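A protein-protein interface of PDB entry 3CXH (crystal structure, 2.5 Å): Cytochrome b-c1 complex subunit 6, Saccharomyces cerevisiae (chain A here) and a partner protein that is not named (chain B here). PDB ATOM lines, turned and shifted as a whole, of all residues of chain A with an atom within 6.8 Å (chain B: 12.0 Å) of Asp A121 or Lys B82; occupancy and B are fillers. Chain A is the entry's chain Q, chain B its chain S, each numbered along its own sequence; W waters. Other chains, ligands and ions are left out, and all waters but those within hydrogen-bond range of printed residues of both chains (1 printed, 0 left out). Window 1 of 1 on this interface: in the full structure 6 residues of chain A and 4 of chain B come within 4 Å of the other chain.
SG of Cys A100 is in hydrogen-bond range of NZ of Lys B82, 3.3 Å away. The side-chain carboxylate (OE2) of Glu A120 lies within salt-bridge range of the side-chain amino group (NZ) of Lys B82, at 2.8 Å. The backbone carbonyl oxygen (O) of Asp A121 sits at hydrogen-bond distance from the side-chain amino group (NZ) of Lys B82, at 2.8 Å. The backbone NH of Lys B82 sits at hydrogen-bond distance from the side-chain carboxylate of Glu A124 (2.8 Å). The side-chain carboxylate (OE2) of Glu A125 is in salt-bridge range of the side-chain amino group (NZ) of Lys B82.
The side-chain sulfur (SG) of Cys A100 lies close to the guanidinium group (NH1) of Arg A103 (3.6 Å). The side-chain sulfur of Cys A122 forms a disulfide with the side-chain sulfur of Cys A100 (2.0 Å). The side-chain carboxylate (OE2) of Glu A120 lies within salt-bridge range of the guanidinium group (NH1) of Arg A103, 3.1 Å away. The side-chain carboxylate (OE1) of Glu A120 lies within hydrogen-bond range of the side-chain amide nitrogen (NE2) of Gln A107 (3.3 Å). The side-chain carboxylate of Asp A121 is in hydrogen-bond range of the backbone NH of Val A123. The backbone carbonyl oxygen of Phe B78 is in hydrogen-bond range of the side-chain hydroxyl of Ser B81, 2.9 Å away.
Among the printed residues, merely in contact across the chains: Glu A124 with Ser B81.
Cys A100 touches one residue of chain B. Val A104 touches none of the printed residues of chain B. Lys A119 touches none of the printed residues of chain B. Glu A120 touches just one residue of chain B: Lys B82 (2.8 Å). Asp A121 touches just one residue of chain B: Lys B82 (2.8 Å). No residue of chain B comes within 4 Å of Cys A122. No residue of chain B comes within 4 Å of Val A123. Glu A124 touches two residues of chain B. Printed residues of chain B within 4 Å of Glu A125: Lys B82. Of the printed residues of chain A, Ser B81 touches Glu A124. Of chain A, only Cys A100 (3.3 Å), Glu A120 (2.8 Å), Asp A121 (2.8 Å), Glu A124 (2.8 Å) and Glu A125 (2.7 Å) come within 4 Å of Lys B82. The nearest residue of chain B that does not touch Asp A121 is Arg B85 (8.2 Å). The nearest printed residue of chain A that does not touch Ser B81 is Glu A125 (8.8 Å).
Along chain B the printed residues that touch a printed residue of chain A span positions 81 to 82.
Water W1 lies within hydrogen-bond range of the side-chain carboxylate (OE1) of Glu A124 (2.8 Å), the backbone NH (N) of Ala B83 (2.9 Å), the backbone NH (N) of Lys B82 (3.0 Å) and the side-chain hydroxyl (OG) of Ser B81 (3.4 Å).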
ATOM      1  N   CYS A 100     -15.390  -2.901 -20.122  1.00  0.00           N
ATOM      2  CA  CYS A 100     -15.361  -3.939 -19.100  1.00  0.00           C
ATOM      3  C   CYS A 100     -15.866  -3.368 -17.781  1.00  0.00           C
ATOM      4  O   CYS A 100     -16.685  -3.990 -17.111  1.00  0.00           O
ATOM      5  CB  CYS A 100     -13.937  -4.480 -18.924  1.00  0.00           C
ATOM      6  SG  CYS A 100     -13.768  -5.813 -17.685  1.00  0.00           S
ATOM      7  N   ARG A 103     -19.630  -3.120 -17.943  1.00  0.00           N
ATOM      8  CA  ARG A 103     -20.212  -4.452 -17.881  1.00  0.00           C
ATOM      9  C   ARG A 103     -20.183  -4.977 -16.443  1.00  0.00           C
ATOM     10  O   ARG A 103     -21.134  -5.615 -15.990  1.00  0.00           O
ATOM     11  CB  ARG A 103     -19.453  -5.387 -18.826  1.00  0.00           C
ATOM     12  CG  ARG A 103     -19.941  -6.826 -18.833  1.00  0.00           C
ATOM     13  CD  ARG A 103     -19.278  -7.638 -19.944  1.00  0.00           C
ATOM     14  NE  ARG A 103     -17.819  -7.632 -19.860  1.00  0.00           N
ATOM     15  CZ  ARG A 103     -17.020  -6.932 -20.663  1.00  0.00           C
ATOM     16  NH1 ARG A 103     -15.704  -6.989 -20.503  1.00  0.00           N
ATOM     17  NH2 ARG A 103     -17.530  -6.173 -21.629  1.00  0.00           N
ATOM     18  N   VAL A 104     -19.108  -4.655 -15.723  1.00  0.00           N
ATOM     19  CA  VAL A 104     -18.935  -5.071 -14.332  1.00  0.00           C
ATOM     20  C   VAL A 104     -19.877  -4.306 -13.401  1.00  0.00           C
ATOM     21  O   VAL A 104     -20.478  -4.891 -12.501  1.00  0.00           O
ATOM     22  CB  VAL A 104     -17.462  -4.884 -13.867  1.00  0.00           C
ATOM     23  CG1 VAL A 104     -17.341  -5.044 -12.359  1.00  0.00           C
ATOM     24  CG2 VAL A 104     -16.571  -5.900 -14.553  1.00  0.00           C
ATOM     25  N   GLN A 107     -23.280  -5.665 -13.453  1.00  0.00           N
ATOM     26  CA  GLN A 107     -23.363  -6.967 -12.793  1.00  0.00           C
ATOM     27  C   GLN A 107     -23.501  -6.803 -11.279  1.00  0.00           C
ATOM     28  O   GLN A 107     -24.206  -7.572 -10.625  1.00  0.00           O
ATOM     29  CB  GLN A 107     -22.118  -7.808 -13.089  1.00  0.00           C
ATOM     30  CG  GLN A 107     -21.985  -8.282 -14.529  1.00  0.00           C
ATOM     31  CD  GLN A 107     -20.708  -9.074 -14.766  1.00  0.00           C
ATOM     32  OE1 GLN A 107     -20.096  -9.591 -13.823  1.00  0.00           O
ATOM     33  NE2 GLN A 107     -20.299  -9.173 -16.029  1.00  0.00           N
ATOM     34  N   TYR A 113     -25.712 -10.969  -6.997  1.00  0.00           N
ATOM     35  CA  TYR A 113     -24.279 -10.843  -7.266  1.00  0.00           C
ATOM     36  C   TYR A 113     -23.424 -11.451  -6.164  1.00  0.00           C
ATOM     37  O   TYR A 113     -22.557 -12.283  -6.435  1.00  0.00           O
ATOM     38  CB  TYR A 113     -23.898  -9.369  -7.449  1.00  0.00           C
ATOM     39  CG  TYR A 113     -22.458  -9.133  -7.865  1.00  0.00           C
ATOM     40  CD1 TYR A 113     -21.569  -8.457  -7.029  1.00  0.00           C
ATOM     41  CD2 TYR A 113     -21.991  -9.565  -9.106  1.00  0.00           C
ATOM     42  CE1 TYR A 113     -20.249  -8.215  -7.421  1.00  0.00           C
ATOM     43  CE2 TYR A 113     -20.675  -9.329  -9.508  1.00  0.00           C
ATOM     44  CZ  TYR A 113     -19.810  -8.653  -8.664  1.00  0.00           C
ATOM     45  OH  TYR A 113     -18.516  -8.406  -9.069  1.00  0.00           O
ATOM     46  N   LYS A 119     -17.341 -14.109 -10.459  1.00  0.00           N
ATOM     47  CA  LYS A 119     -17.498 -12.706 -10.867  1.00  0.00           C
ATOM     48  C   LYS A 119     -16.360 -12.188 -11.754  1.00  0.00           C
ATOM     49  O   LYS A 119     -15.185 -12.481 -11.517  1.00  0.00           O
ATOM     50  CB  LYS A 119     -17.601 -11.808  -9.629  1.00  0.00           C
ATOM     51  CG  LYS A 119     -18.218 -12.473  -8.407  1.00  0.00           C
ATOM     52  CD  LYS A 119     -18.179 -11.556  -7.189  1.00  0.00           C
ATOM     53  CE  LYS A 119     -18.388 -12.330  -5.888  1.00  0.00           C
ATOM     54  NZ  LYS A 119     -19.645 -13.129  -5.884  1.00  0.00           N
ATOM     55  N   GLU A 120     -16.717 -11.369 -12.738  1.00  0.00           N
ATOM     56  CA  GLU A 120     -15.740 -10.803 -13.662  1.00  0.00           C
ATOM     57  C   GLU A 120     -15.060  -9.538 -13.149  1.00  0.00           C
ATOM     58  O   GLU A 120     -15.704  -8.691 -12.536  1.00  0.00           O
ATOM     59  CB  GLU A 120     -16.401 -10.500 -15.014  1.00  0.00           C
ATOM     60  CG  GLU A 120     -15.462  -9.833 -16.031  1.00  0.00           C
ATOM     61  CD  GLU A 120     -16.121  -9.490 -17.364  1.00  0.00           C
ATOM     62  OE1 GLU A 120     -17.364  -9.570 -17.478  1.00  0.00           O
ATOM     63  OE2 GLU A 120     -15.386  -9.128 -18.307  1.00  0.00           O
ATOM     64  N   ASP A 121     -13.745  -9.451 -13.356  1.00  0.00           N
ATOM     65  CA  ASP A 121     -12.970  -8.262 -12.988  1.00  0.00           C
ATOM     66  C   ASP A 121     -12.304  -7.744 -14.261  1.00  0.00           C
ATOM     67  O   ASP A 121     -12.420  -8.366 -15.311  1.00  0.00           O
ATOM     68  CB  ASP A 121     -11.953  -8.523 -11.850  1.00  0.00           C
ATOM     69  CG  ASP A 121     -10.872  -9.546 -12.209  1.00  0.00           C
ATOM     70  OD1 ASP A 121     -10.928 -10.675 -11.668  1.00  0.00           O
ATOM     71  OD2 ASP A 121      -9.938  -9.211 -12.979  1.00  0.00           O
ATOM     72  N   CYS A 122     -11.623  -6.608 -14.183  1.00  0.00           N
ATOM     73  CA  CYS A 122     -10.997  -6.036 -15.369  1.00  0.00           C
ATOM     74  C   CYS A 122      -9.491  -5.838 -15.268  1.00  0.00           C
ATOM     75  O   CYS A 122      -8.930  -4.920 -15.877  1.00  0.00           O
ATOM     76  CB  CYS A 122     -11.689  -4.713 -15.731  1.00  0.00           C
ATOM     77  SG  CYS A 122     -13.497  -4.852 -15.909  1.00  0.00           S
ATOM     78  N   VAL A 123      -8.837  -6.717 -14.511  1.00  0.00           N
ATOM     79  CA  VAL A 123      -7.394  -6.671 -14.328  1.00  0.00           C
ATOM     80  C   VAL A 123      -6.704  -6.884 -15.666  1.00  0.00           C
ATOM     81  O   VAL A 123      -5.759  -6.181 -16.013  1.00  0.00           O
ATOM     82  CB  VAL A 123      -6.937  -7.756 -13.340  1.00  0.00           C
ATOM     83  CG1 VAL A 123      -5.415  -7.900 -13.359  1.00  0.00           C
ATOM     84  CG2 VAL A 123      -7.407  -7.398 -11.952  1.00  0.00           C
ATOM     85  N   GLU A 124      -7.206  -7.849 -16.425  1.00  0.00           N
ATOM     86  CA  GLU A 124      -6.643  -8.166 -17.723  1.00  0.00           C
ATOM     87  C   GLU A 124      -6.652  -6.923 -18.628  1.00  0.00           C
ATOM     88  O   GLU A 124      -5.600  -6.495 -19.110  1.00  0.00           O
ATOM     89  CB  GLU A 124      -7.429  -9.319 -18.341  1.00  0.00           C
ATOM     90  CG  GLU A 124      -6.753  -9.992 -19.514  1.00  0.00           C
ATOM     91  CD  GLU A 124      -7.581 -11.145 -20.055  1.00  0.00           C
ATOM     92  OE1 GLU A 124      -8.583 -10.877 -20.753  1.00  0.00           O
ATOM     93  OE2 GLU A 124      -7.251 -12.318 -19.768  1.00  0.00           O
ATOM     94  N   GLU A 125      -7.829  -6.318 -18.805  1.00  0.00           N
ATOM     95  CA  GLU A 125      -7.969  -5.124 -19.640  1.00  0.00           C
ATOM     96  C   GLU A 125      -7.127  -3.985 -19.088  1.00  0.00           C
ATOM     97  O   GLU A 125      -6.553  -3.199 -19.842  1.00  0.00           O
ATOM     98  CB  GLU A 125      -9.432  -4.684 -19.744  1.00  0.00           C
ATOM     99  CG  GLU A 125     -10.340  -5.635 -20.497  1.00  0.00           C
ATOM    100  CD  GLU A 125     -10.827  -6.803 -19.656  1.00  0.00           C
ATOM    101  OE1 GLU A 125     -10.523  -6.859 -18.448  1.00  0.00           O
ATOM    102  OE2 GLU A 125     -11.538  -7.669 -20.205  1.00  0.00           O
ATOM    103  N   GLU B  74       1.885 -21.397 -24.890  1.00  0.00           N
ATOM    104  CA  GLU B  74       0.762 -20.595 -25.345  1.00  0.00           C
ATOM    105  C   GLU B  74      -0.551 -21.152 -24.819  1.00  0.00           C
ATOM    106  O   GLU B  74      -1.432 -20.393 -24.415  1.00  0.00           O
ATOM    107  CB  GLU B  74       0.756 -20.530 -26.863  1.00  0.00           C
ATOM    108  CG  GLU B  74       1.888 -19.667 -27.405  1.00  0.00           C
ATOM    109  CD  GLU B  74       2.213 -19.937 -28.865  1.00  0.00           C
ATOM    110  OE1 GLU B  74       3.152 -19.284 -29.382  1.00  0.00           O
ATOM    111  OE2 GLU B  74       1.556 -20.810 -29.486  1.00  0.00           O
ATOM    112  N   TYR B  75      -0.665 -22.475 -24.783  1.00  0.00           N
ATOM    113  CA  TYR B  75      -1.872 -23.117 -24.276  1.00  0.00           C
ATOM    114  C   TYR B  75      -2.078 -22.706 -22.813  1.00  0.00           C
ATOM    115  O   TYR B  75      -3.197 -22.410 -22.402  1.00  0.00           O
ATOM    116  CB  TYR B  75      -1.765 -24.644 -24.409  1.00  0.00           C
ATOM    117  CG  TYR B  75      -3.015 -25.388 -23.994  1.00  0.00           C
ATOM    118  CD1 TYR B  75      -4.273 -24.966 -24.419  1.00  0.00           C
ATOM    119  CD2 TYR B  75      -2.942 -26.491 -23.148  1.00  0.00           C
ATOM    120  CE1 TYR B  75      -5.436 -25.622 -24.006  1.00  0.00           C
ATOM    121  CE2 TYR B  75      -4.095 -27.157 -22.726  1.00  0.00           C
ATOM    122  CZ  TYR B  75      -5.339 -26.713 -23.159  1.00  0.00           C
ATOM    123  OH  TYR B  75      -6.483 -27.348 -22.735  1.00  0.00           O
ATOM    124  N   ASN B  76      -0.984 -22.639 -22.057  1.00  0.00           N
ATOM    125  CA  ASN B  76      -1.010 -22.245 -20.645  1.00  0.00           C
ATOM    126  C   ASN B  76      -1.484 -20.805 -20.514  1.00  0.00           C
ATOM    127  O   ASN B  76      -2.293 -20.482 -19.647  1.00  0.00           O
ATOM    128  CB  ASN B  76       0.395 -22.353 -20.037  1.00  0.00           C
ATOM    129  CG  ASN B  76       0.414 -22.055 -18.548  1.00  0.00           C
ATOM    130  OD1 ASN B  76       0.876 -20.998 -18.111  1.00  0.00           O
ATOM    131  ND2 ASN B  76      -0.082 -22.991 -17.761  1.00  0.00           N
ATOM    132  N   GLU B  77      -0.949 -19.948 -21.380  1.00  0.00           N
ATOM    133  CA  GLU B  77      -1.278 -18.528 -21.404  1.00  0.00           C
ATOM    134  C   GLU B  77      -2.778 -18.333 -21.619  1.00  0.00           C
ATOM    135  O   GLU B  77      -3.415 -17.527 -20.930  1.00  0.00           O
ATOM    136  CB  GLU B  77      -0.488 -17.844 -22.519  1.00  0.00           C
ATOM    137  CG  GLU B  77      -0.442 -16.330 -22.429  1.00  0.00           C
ATOM    138  CD  GLU B  77       0.378 -15.700 -23.550  1.00  0.00           C
ATOM    139  OE1 GLU B  77       1.221 -16.407 -24.164  1.00  0.00           O
ATOM    140  OE2 GLU B  77       0.179 -14.490 -23.814  1.00  0.00           O
ATOM    141  N   PHE B  78      -3.333 -19.090 -22.565  1.00  0.00           N
ATOM    142  CA  PHE B  78      -4.755 -19.033 -22.877  1.00  0.00           C
ATOM    143  C   PHE B  78      -5.573 -19.575 -21.699  1.00  0.00           C
ATOM    144  O   PHE B  78      -6.538 -18.946 -21.257  1.00  0.00           O
ATOM    145  CB  PHE B  78      -5.025 -19.825 -24.163  1.00  0.00           C
ATOM    146  CG  PHE B  78      -6.461 -20.220 -24.356  1.00  0.00           C
ATOM    147  CD1 PHE B  78      -7.392 -19.307 -24.831  1.00  0.00           C
ATOM    148  CD2 PHE B  78      -6.885 -21.510 -24.042  1.00  0.00           C
ATOM    149  CE1 PHE B  78      -8.732 -19.672 -24.990  1.00  0.00           C
ATOM    150  CE2 PHE B  78      -8.219 -21.890 -24.194  1.00  0.00           C
ATOM    151  CZ  PHE B  78      -9.146 -20.967 -24.669  1.00  0.00           C
ATOM    152  N   LEU B  79      -5.171 -20.730 -21.180  1.00  0.00           N
ATOM    153  CA  LEU B  79      -5.867 -21.345 -20.059  1.00  0.00           C
ATOM    154  C   LEU B  79      -6.016 -20.415 -18.864  1.00  0.00           C
ATOM    155  O   LEU B  79      -7.002 -20.503 -18.132  1.00  0.00           O
ATOM    156  CB  LEU B  79      -5.158 -22.623 -19.610  1.00  0.00           C
ATOM    157  CG  LEU B  79      -5.519 -23.913 -20.344  1.00  0.00           C
ATOM    158  CD1 LEU B  79      -4.750 -25.087 -19.734  1.00  0.00           C
ATOM    159  CD2 LEU B  79      -7.012 -24.141 -20.235  1.00  0.00           C
ATOM    160  N   TYR B  80      -5.047 -19.522 -18.675  1.00  0.00           N
ATOM    161  CA  TYR B  80      -5.089 -18.588 -17.554  1.00  0.00           C
ATOM    162  C   TYR B  80      -5.565 -17.151 -17.848  1.00  0.00           C
ATOM    163  O   TYR B  80      -5.471 -16.263 -17.002  1.00  0.00           O
ATOM    164  CB  TYR B  80      -3.763 -18.631 -16.788  1.00  0.00           C
ATOM    165  CG  TYR B  80      -3.690 -19.865 -15.914  1.00  0.00           C
ATOM    166  CD1 TYR B  80      -3.135 -21.061 -16.392  1.00  0.00           C
ATOM    167  CD2 TYR B  80      -4.250 -19.865 -14.635  1.00  0.00           C
ATOM    168  CE1 TYR B  80      -3.153 -22.227 -15.618  1.00  0.00           C
ATOM    169  CE2 TYR B  80      -4.268 -21.021 -13.852  1.00  0.00           C
ATOM    170  CZ  TYR B  80      -3.721 -22.201 -14.347  1.00  0.00           C
ATOM    171  OH  TYR B  80      -3.746 -23.341 -13.565  1.00  0.00           O
ATOM    172  N   SER B  81      -6.105 -16.946 -19.047  1.00  0.00           N
ATOM    173  CA  SER B  81      -6.641 -15.650 -19.448  1.00  0.00           C
ATOM    174  C   SER B  81      -8.159 -15.749 -19.275  1.00  0.00           C
ATOM    175  O   SER B  81      -8.681 -16.838 -19.017  1.00  0.00           O
ATOM    176  CB  SER B  81      -6.277 -15.331 -20.909  1.00  0.00           C
ATOM    177  OG  SER B  81      -6.954 -16.175 -21.832  1.00  0.00           O
ATOM    178  N   LYS B  82      -8.858 -14.617 -19.370  1.00  0.00           N
ATOM    179  CA  LYS B  82     -10.317 -14.594 -19.227  1.00  0.00           C
ATOM    180  C   LYS B  82     -11.019 -15.539 -20.196  1.00  0.00           C
ATOM    181  O   LYS B  82     -11.950 -16.250 -19.824  1.00  0.00           O
ATOM    182  CB  LYS B  82     -10.865 -13.197 -19.488  1.00  0.00           C
ATOM    183  CG  LYS B  82     -10.991 -12.303 -18.285  1.00  0.00           C
ATOM    184  CD  LYS B  82     -11.868 -11.127 -18.659  1.00  0.00           C
ATOM    185  CE  LYS B  82     -11.767 -10.021 -17.655  1.00  0.00           C
ATOM    186  NZ  LYS B  82     -12.618  -8.890 -18.077  1.00  0.00           N
ATOM    187  N   ALA B  83     -10.576 -15.509 -21.449  1.00  0.00           N
ATOM    188  CA  ALA B  83     -11.145 -16.332 -22.506  1.00  0.00           C
ATOM    189  C   ALA B  83     -10.971 -17.829 -22.271  1.00  0.00           C
ATOM    190  O   ALA B  83     -11.699 -18.638 -22.851  1.00  0.00           O
ATOM    191  CB  ALA B  83     -10.534 -15.938 -23.852  1.00  0.00           C
ATOM    192  N   GLY B  84     -10.028 -18.203 -21.413  1.00  0.00           N
ATOM    193  CA  GLY B  84      -9.796 -19.616 -21.180  1.00  0.00           C
ATOM    194  C   GLY B  84     -10.286 -20.242 -19.891  1.00  0.00           C
ATOM    195  O   GLY B  84     -10.064 -21.434 -19.696  1.00  0.00           O
ATOM    196  N   ARG B  85     -10.964 -19.488 -19.028  1.00  0.00           N
ATOM    197  CA  ARG B  85     -11.427 -20.058 -17.760  1.00  0.00           C
ATOM    198  C   ARG B  85     -12.437 -21.191 -17.878  1.00  0.00           C
ATOM    199  O   ARG B  85     -12.537 -22.035 -16.992  1.00  0.00           O
ATOM    200  CB  ARG B  85     -11.941 -18.980 -16.804  1.00  0.00           C
ATOM    201  CG  ARG B  85     -12.988 -18.062 -17.382  1.00  0.00           C
ATOM    202  CD  ARG B  85     -13.534 -17.133 -16.305  1.00  0.00           C
ATOM    203  NE  ARG B  85     -14.280 -17.874 -15.288  1.00  0.00           N
ATOM    204  CZ  ARG B  85     -15.509 -18.356 -15.463  1.00  0.00           C
ATOM    205  NH1 ARG B  85     -16.107 -19.023 -14.482  1.00  0.00           N
ATOM    206  NH2 ARG B  85     -16.145 -18.159 -16.615  1.00  0.00           N
ATOM    207  N   GLU B  86     -13.167 -21.227 -18.983  1.00  0.00           N
ATOM    208  CA  GLU B  86     -14.150 -22.276 -19.200  1.00  0.00           C
ATOM    209  C   GLU B  86     -13.426 -23.600 -19.459  1.00  0.00           C
ATOM    210  O   GLU B  86     -13.703 -24.608 -18.806  1.00  0.00           O
ATOM    211  CB  GLU B  86     -15.059 -21.911 -20.372  1.00  0.00           C
ATOM    212  CG  GLU B  86     -16.287 -22.794 -20.500  1.00  0.00           C
ATOM    213  CD  GLU B  86     -17.188 -22.410 -21.667  1.00  0.00           C
ATOM    214  OE1 GLU B  86     -16.815 -21.512 -22.466  1.00  0.00           O
ATOM    215  OE2 GLU B  86     -18.277 -23.018 -21.780  1.00  0.00           O
ATOM    216  N   GLU B  87     -12.476 -23.584 -20.393  1.00  0.00           N
ATOM    217  CA  GLU B  87     -11.703 -24.777 -20.711  1.00  0.00           C
ATOM    218  C   GLU B  87     -10.786 -25.132 -19.534  1.00  0.00           C
ATOM    219  O   GLU B  87     -10.439 -26.297 -19.338  1.00  0.00           O
ATOM    220  CB  GLU B  87     -10.887 -24.574 -21.989  1.00  0.00           C
ATOM    221  CG  GLU B  87     -10.271 -25.864 -22.521  1.00  0.00           C
ATOM    222  CD  GLU B  87      -9.669 -25.730 -23.913  1.00  0.00           C
ATOM    223  OE1 GLU B  87     -10.073 -24.816 -24.669  1.00  0.00           O
ATOM    224  OE2 GLU B  87      -8.796 -26.557 -24.257  1.00  0.00           O
ATOM    225  N   LEU B  88     -10.432 -24.126 -18.736  1.00  0.00           N
ATOM    226  CA  LEU B  88      -9.577 -24.327 -17.571  1.00  0.00           C
ATOM    227  C   LEU B  88     -10.303 -25.166 -16.522  1.00  0.00           C
ATOM    228  O   LEU B  88      -9.724 -26.100 -15.977  1.00  0.00           O
ATOM    229  CB  LEU B  88      -9.141 -22.973 -16.993  1.00  0.00           C
ATOM    230  CG  LEU B  88      -8.056 -22.839 -15.912  1.00  0.00           C
ATOM    231  CD1 LEU B  88      -8.620 -23.049 -14.523  1.00  0.00           C
ATOM    232  CD2 LEU B  88      -6.911 -23.786 -16.192  1.00  0.00           C
ATOM    233  N   GLU B  89     -11.574 -24.855 -16.266  1.00  0.00           N
ATOM    234  CA  GLU B  89     -12.372 -25.603 -15.288  1.00  0.00           C
ATOM    235  C   GLU B  89     -12.485 -27.076 -15.679  1.00  0.00           C
ATOM    236  O   GLU B  89     -12.490 -27.966 -14.827  1.00  0.00           O
ATOM    237  CB  GLU B  89     -13.786 -25.019 -15.168  1.00  0.00           C
ATOM    238  CG  GLU B  89     -13.879 -23.647 -14.502  1.00  0.00           C
ATOM    239  CD  GLU B  89     -15.321 -23.162 -14.344  1.00  0.00           C
ATOM    240  OE1 GLU B  89     -16.055 -23.111 -15.360  1.00  0.00           O
ATOM    241  OE2 GLU B  89     -15.719 -22.831 -13.204  1.00  0.00           O
ATOM    242  N   ARG B  90     -12.567 -27.311 -16.983  1.00  0.00           N
ATOM    243  CA  ARG B  90     -12.693 -28.646 -17.542  1.00  0.00           C
ATOM    244  C   ARG B  90     -11.409 -29.465 -17.403  1.00  0.00           C
ATOM    245  O   ARG B  90     -11.317 -30.344 -16.547  1.00  0.00           O
ATOM    246  CB  ARG B  90     -13.087 -28.530 -19.015  1.00  0.00           C
ATOM    247  CG  ARG B  90     -13.515 -29.826 -19.679  1.00  0.00           C
ATOM    248  CD  ARG B  90     -13.717 -29.610 -21.177  1.00  0.00           C
ATOM    249  NE  ARG B  90     -14.562 -28.445 -21.442  1.00  0.00           N
ATOM    250  CZ  ARG B  90     -14.261 -27.472 -22.299  1.00  0.00           C
ATOM    251  NH1 ARG B  90     -15.093 -26.451 -22.463  1.00  0.00           N
ATOM    252  NH2 ARG B  90     -13.132 -27.520 -22.998  1.00  0.00           N
HETATM  253  O   HOH W   1      -8.778 -13.321 -22.113  1.00  0.00           O
